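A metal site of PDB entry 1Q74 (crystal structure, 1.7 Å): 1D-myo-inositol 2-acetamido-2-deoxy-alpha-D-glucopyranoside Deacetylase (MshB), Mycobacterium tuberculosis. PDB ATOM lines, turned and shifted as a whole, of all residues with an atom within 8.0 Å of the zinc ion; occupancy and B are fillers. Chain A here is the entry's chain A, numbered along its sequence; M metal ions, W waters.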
ATOM      1  N   HIS A  11      17.565 -25.501   9.745  1.00  0.00           N
ATOM      2  CA  HIS A  11      18.084 -24.107   9.681  1.00  0.00           C
ATOM      3  C   HIS A  11      18.874 -23.775  10.917  1.00  0.00           C
ATOM      4  O   HIS A  11      18.726 -24.389  11.971  1.00  0.00           O
ATOM      5  CB  HIS A  11      16.891 -23.147   9.488  1.00  0.00           C
ATOM      6  CG  HIS A  11      16.456 -23.052   8.072  1.00  0.00           C
ATOM      7  ND1 HIS A  11      17.202 -22.370   7.125  1.00  0.00           N
ATOM      8  CD2 HIS A  11      15.430 -23.617   7.404  1.00  0.00           C
ATOM      9  CE1 HIS A  11      16.607 -22.451   5.964  1.00  0.00           C
ATOM     10  NE2 HIS A  11      15.552 -23.222   6.076  1.00  0.00           N
ATOM     11  N   ALA A  12      19.716 -22.756  10.825  1.00  0.00           N
ATOM     12  CA  ALA A  12      20.568 -22.358  11.923  1.00  0.00           C
ATOM     13  C   ALA A  12      19.909 -21.455  12.951  1.00  0.00           C
ATOM     14  O   ALA A  12      20.050 -21.691  14.146  1.00  0.00           O
ATOM     15  CB  ALA A  12      21.655 -21.654  11.368  1.00  0.00           C
ATOM     16  N   HIS A  13      19.173 -20.436  12.506  1.00  0.00           N
ATOM     17  CA  HIS A  13      18.668 -19.429  13.379  1.00  0.00           C
ATOM     18  C   HIS A  13      17.171 -19.116  13.104  1.00  0.00           C
ATOM     19  O   HIS A  13      16.669 -19.346  12.016  1.00  0.00           O
ATOM     20  CB  HIS A  13      19.386 -18.095  13.162  1.00  0.00           C
ATOM     21  CG  HIS A  13      20.877 -18.172  13.150  1.00  0.00           C
ATOM     22  ND1 HIS A  13      21.643 -17.941  12.025  1.00  0.00           N
ATOM     23  CD2 HIS A  13      21.749 -18.430  14.153  1.00  0.00           C
ATOM     24  CE1 HIS A  13      22.925 -18.045  12.345  1.00  0.00           C
ATOM     25  NE2 HIS A  13      23.020 -18.355  13.626  1.00  0.00           N
ATOM     26  N   PRO A  14      16.484 -18.493  14.060  1.00  0.00           N
ATOM     27  CA  PRO A  14      15.124 -18.060  13.792  1.00  0.00           C
ATOM     28  C   PRO A  14      15.074 -16.910  12.811  1.00  0.00           C
ATOM     29  O   PRO A  14      15.625 -15.857  13.123  1.00  0.00           O
ATOM     30  CB  PRO A  14      14.620 -17.543  15.165  1.00  0.00           C
ATOM     31  CG  PRO A  14      15.574 -18.069  16.120  1.00  0.00           C
ATOM     32  CD  PRO A  14      16.916 -18.209  15.443  1.00  0.00           C
ATOM     33  N   ASP A  15      14.409 -17.107  11.675  1.00  0.00           N
ATOM     34  CA  ASP A  15      14.339 -16.189  10.530  1.00  0.00           C
ATOM     35  C   ASP A  15      14.812 -16.860   9.258  1.00  0.00           C
ATOM     36  O   ASP A  15      14.256 -16.590   8.205  1.00  0.00           O
ATOM     37  CB  ASP A  15      14.912 -14.754  10.619  1.00  0.00           C
ATOM     38  CG  ASP A  15      16.366 -14.654  10.760  1.00  0.00           C
ATOM     39  OD1 ASP A  15      17.129 -15.639  10.613  1.00  0.00           O
ATOM     40  OD2 ASP A  15      16.855 -13.533  11.048  1.00  0.00           O
ATOM     41  N   ASP A  16      15.797 -17.738   9.398  1.00  0.00           N
ATOM     42  CA  ASP A  16      16.371 -18.368   8.199  1.00  0.00           C
ATOM     43  C   ASP A  16      15.350 -19.192   7.413  1.00  0.00           C
ATOM     44  O   ASP A  16      15.381 -19.248   6.186  1.00  0.00           O
ATOM     45  CB  ASP A  16      17.577 -19.240   8.580  1.00  0.00           C
ATOM     46  CG  ASP A  16      18.772 -18.440   8.903  1.00  0.00           C
ATOM     47  OD1 ASP A  16      19.182 -17.578   8.075  1.00  0.00           O
ATOM     48  OD2 ASP A  16      19.407 -18.640   9.937  1.00  0.00           O
ATOM     49  N   GLU A  17      14.431 -19.862   8.107  1.00  0.00           N
ATOM     50  CA  GLU A  17      13.398 -20.635   7.471  1.00  0.00           C
ATOM     51  C   GLU A  17      12.494 -19.812   6.558  1.00  0.00           C
ATOM     52  O   GLU A  17      12.060 -20.284   5.479  1.00  0.00           O
ATOM     53  CB  GLU A  17      12.529 -21.387   8.516  1.00  0.00           C
ATOM     54  CG  GLU A  17      11.483 -20.566   9.266  1.00  0.00           C
ATOM     55  CD  GLU A  17      11.978 -19.424  10.095  1.00  0.00           C
ATOM     56  OE1 GLU A  17      13.123 -19.524  10.656  1.00  0.00           O
ATOM     57  OE2 GLU A  17      11.242 -18.416  10.228  1.00  0.00           O
ATOM     58  N   LEU A  19      13.344 -16.504   5.455  1.00  0.00           N
ATOM     59  CA  LEU A  19      14.219 -15.869   4.446  1.00  0.00           C
ATOM     60  C   LEU A  19      14.512 -16.800   3.299  1.00  0.00           C
ATOM     61  O   LEU A  19      14.455 -16.391   2.126  1.00  0.00           O
ATOM     62  CB  LEU A  19      15.530 -15.416   5.099  1.00  0.00           C
ATOM     63  CG  LEU A  19      15.439 -14.239   6.059  1.00  0.00           C
ATOM     64  CD1 LEU A  19      16.688 -14.209   6.983  1.00  0.00           C
ATOM     65  CD2 LEU A  19      15.223 -12.870   5.315  1.00  0.00           C
ATOM     66  N   SER A  20      14.825 -18.044   3.602  1.00  0.00           N
ATOM     67  CA  SER A  20      15.212 -19.002   2.545  1.00  0.00           C
ATOM     68  C   SER A  20      14.017 -19.744   1.897  1.00  0.00           C
ATOM     69  O   SER A  20      13.935 -19.858   0.693  1.00  0.00           O
ATOM     70  CB  SER A  20      16.089 -20.098   3.121  1.00  0.00           C
ATOM     71  OG  SER A  20      17.404 -19.654   3.533  1.00  0.00           O
ATOM     72  N   THR A  41      19.596 -23.209  16.846  1.00  0.00           N
ATOM     73  CA  THR A  41      19.889 -22.285  17.941  1.00  0.00           C
ATOM     74  C   THR A  41      18.735 -21.320  18.161  1.00  0.00           C
ATOM     75  O   THR A  41      17.861 -21.185  17.285  1.00  0.00           O
ATOM     76  CB  THR A  41      21.188 -21.494  17.639  1.00  0.00           C
ATOM     77  OG1 THR A  41      20.912 -20.508  16.621  1.00  0.00           O
ATOM     78  CG2 THR A  41      22.354 -22.393  17.202  1.00  0.00           C
ATOM     79  N   ARG A  68      12.968 -14.513  20.879  1.00  0.00           N
ATOM     80  CA  ARG A  68      12.831 -14.977  19.533  1.00  0.00           C
ATOM     81  C   ARG A  68      12.050 -16.290  19.328  1.00  0.00           C
ATOM     82  O   ARG A  68      11.548 -16.596  18.246  1.00  0.00           O
ATOM     83  CB  ARG A  68      14.169 -14.970  18.791  1.00  0.00           C
ATOM     84  CG  ARG A  68      14.663 -13.610  18.606  1.00  0.00           C
ATOM     85  CD  ARG A  68      16.091 -13.552  18.043  1.00  0.00           C
ATOM     86  NE  ARG A  68      16.212 -13.999  16.648  1.00  0.00           N
ATOM     87  CZ  ARG A  68      17.368 -14.123  15.952  1.00  0.00           C
ATOM     88  NH1 ARG A  68      18.539 -13.888  16.512  1.00  0.00           N
ATOM     89  NH2 ARG A  68      17.344 -14.458  14.659  1.00  0.00           N
ATOM     90  N   ASP A  95      24.030 -19.944  19.445  1.00  0.00           N
ATOM     91  CA  ASP A  95      24.603 -19.415  18.206  1.00  0.00           C
ATOM     92  C   ASP A  95      25.836 -18.552  18.411  1.00  0.00           C
ATOM     93  O   ASP A  95      26.141 -18.143  19.537  1.00  0.00           O
ATOM     94  CB  ASP A  95      23.626 -18.575  17.468  1.00  0.00           C
ATOM     95  CG  ASP A  95      22.963 -17.609  18.327  1.00  0.00           C
ATOM     96  OD1 ASP A  95      22.305 -18.139  19.258  1.00  0.00           O
ATOM     97  OD2 ASP A  95      22.931 -16.368  18.069  1.00  0.00           O
ATOM     98  N   TYR A 136      21.330 -25.806   4.127  1.00  0.00           N
ATOM     99  CA  TYR A 136      22.237 -24.954   3.359  1.00  0.00           C
ATOM    100  C   TYR A 136      23.245 -25.770   2.574  1.00  0.00           C
ATOM    101  O   TYR A 136      23.479 -26.942   2.844  1.00  0.00           O
ATOM    102  CB  TYR A 136      23.032 -24.011   4.247  1.00  0.00           C
ATOM    103  CG  TYR A 136      22.199 -23.352   5.312  1.00  0.00           C
ATOM    104  CD1 TYR A 136      21.244 -22.426   4.935  1.00  0.00           C
ATOM    105  CD2 TYR A 136      22.252 -23.770   6.613  1.00  0.00           C
ATOM    106  CE1 TYR A 136      20.439 -21.822   5.860  1.00  0.00           C
ATOM    107  CE2 TYR A 136      21.431 -23.172   7.562  1.00  0.00           C
ATOM    108  CZ  TYR A 136      20.528 -22.197   7.182  1.00  0.00           C
ATOM    109  OH  TYR A 136      19.652 -21.643   8.122  1.00  0.00           O
ATOM    110  N   GLY A 140      27.170 -22.585   3.632  1.00  0.00           N
ATOM    111  CA  GLY A 140      26.205 -21.975   4.528  1.00  0.00           C
ATOM    112  C   GLY A 140      25.433 -20.807   3.951  1.00  0.00           C
ATOM    113  O   GLY A 140      24.814 -20.055   4.666  1.00  0.00           O
ATOM    114  N   HIS A 144      28.119 -17.921   7.244  1.00  0.00           N
ATOM    115  CA  HIS A 144      27.924 -17.750   8.672  1.00  0.00           C
ATOM    116  C   HIS A 144      28.328 -19.109   9.320  1.00  0.00           C
ATOM    117  O   HIS A 144      27.927 -20.129   8.846  1.00  0.00           O
ATOM    118  CB  HIS A 144      26.499 -17.352   9.020  1.00  0.00           C
ATOM    119  CG  HIS A 144      26.319 -16.995  10.453  1.00  0.00           C
ATOM    120  ND1 HIS A 144      25.946 -15.734  10.866  1.00  0.00           N
ATOM    121  CD2 HIS A 144      26.576 -17.689  11.589  1.00  0.00           C
ATOM    122  CE1 HIS A 144      25.880 -15.702  12.185  1.00  0.00           C
ATOM    123  NE2 HIS A 144      26.274 -16.869  12.656  1.00  0.00           N
ATOM    124  N   ASP A 146      27.443 -20.805  11.897  1.00  0.00           N
ATOM    125  CA  ASP A 146      26.277 -21.624  12.241  1.00  0.00           C
ATOM    126  C   ASP A 146      25.573 -22.216  11.035  1.00  0.00           C
ATOM    127  O   ASP A 146      25.093 -23.326  11.154  1.00  0.00           O
ATOM    128  CB  ASP A 146      25.209 -20.861  13.084  1.00  0.00           C
ATOM    129  CG  ASP A 146      25.683 -20.503  14.451  1.00  0.00           C
ATOM    130  OD1 ASP A 146      26.414 -21.278  15.132  1.00  0.00           O
ATOM    131  OD2 ASP A 146      25.319 -19.437  14.980  1.00  0.00           O
ATOM    132  N   HIS A 147      25.587 -21.534   9.875  1.00  0.00           N
ATOM    133  CA  HIS A 147      24.970 -22.069   8.690  1.00  0.00           C
ATOM    134  C   HIS A 147      25.891 -23.204   8.148  1.00  0.00           C
ATOM    135  O   HIS A 147      25.416 -24.263   7.763  1.00  0.00           O
ATOM    136  CB  HIS A 147      24.670 -21.059   7.601  1.00  0.00           C
ATOM    137  CG  HIS A 147      23.565 -20.089   7.925  1.00  0.00           C
ATOM    138  ND1 HIS A 147      22.946 -19.302   6.992  1.00  0.00           N
ATOM    139  CD2 HIS A 147      22.945 -19.806   9.073  1.00  0.00           C
ATOM    140  CE1 HIS A 147      22.092 -18.472   7.576  1.00  0.00           C
ATOM    141  NE2 HIS A 147      22.036 -18.770   8.837  1.00  0.00           N
ATOM    142  N   THR A 150      25.368 -26.192  10.419  1.00  0.00           N
ATOM    143  CA  THR A 150      24.090 -26.841  10.151  1.00  0.00           C
ATOM    144  C   THR A 150      24.205 -27.742   8.934  1.00  0.00           C
ATOM    145  O   THR A 150      23.642 -28.859   8.903  1.00  0.00           O
ATOM    146  CB  THR A 150      23.012 -25.752   9.904  1.00  0.00           C
ATOM    147  OG1 THR A 150      22.806 -24.937  11.091  1.00  0.00           O
ATOM    148  CG2 THR A 150      21.686 -26.391   9.621  1.00  0.00           C
ATOM    149  N   LEU A 259      17.525  -6.633   6.341  1.00  0.00           N
ATOM    150  CA  LEU A 259      18.009  -6.902   7.687  1.00  0.00           C
ATOM    151  C   LEU A 259      18.554  -5.561   8.196  1.00  0.00           C
ATOM    152  O   LEU A 259      18.414  -4.546   7.513  1.00  0.00           O
ATOM    153  CB  LEU A 259      19.080  -7.962   7.670  1.00  0.00           C
ATOM    154  CG  LEU A 259      18.722  -9.283   7.031  1.00  0.00           C
ATOM    155  CD1 LEU A 259      19.847 -10.268   7.164  1.00  0.00           C
ATOM    156  CD2 LEU A 259      17.459  -9.862   7.625  1.00  0.00           C
HETATM  157 ZN    ZN M   1      21.072 -17.402  10.071  1.00  0.00          ZN
HETATM  158  O   HOH W   1      22.687 -15.792   9.730  1.00  0.00           O
HETATM  159  O   HOH W   2      19.963 -15.594  10.677  1.00  0.00           O
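A ring nitrogen (ND1) of His 147 sits at hydrogen-bond distance from the backbone carbonyl oxygen (O) of Gly 140, 3.1 Å away.
A ring nitrogen (NE2) of His 13 is in hydrogen-bond range of the side-chain carboxylate (OD2) of Asp 146 (2.9 Å).
The side-chain hydroxyl (OG) of Ser 20 lies close to the backbone carbonyl oxygen (O) of Asp 16, 3.4 Å away.
Within 4 Å of the zinc ion: His 13, Asp 16 and His 147.
The nearest printed residue that does not touch the zinc ion is Asp 15 (4.4 Å).
The side-chain carboxylate (OD2) of Asp 16 binds the zinc ion, 2.1 Å away.
The zinc ion is bound by NE2 of His 147, 2.1 Å away.
The zinc ion is bound by ND1 of His 13 (2.1 Å).
Water W2 is bound to the zinc ion (2.2 Å).
Water W1 is bound to the zinc ion (2.3 Å).
The zinc ion has five donor atoms within binding distance.
Slightly farther from the zinc ion lies the side-chain carboxylate (OD1) of Asp 16 (2.8 Å).
Water W2 lies within hydrogen-bond range of OD1 of Asp 15 and OD1 of Asp 16.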
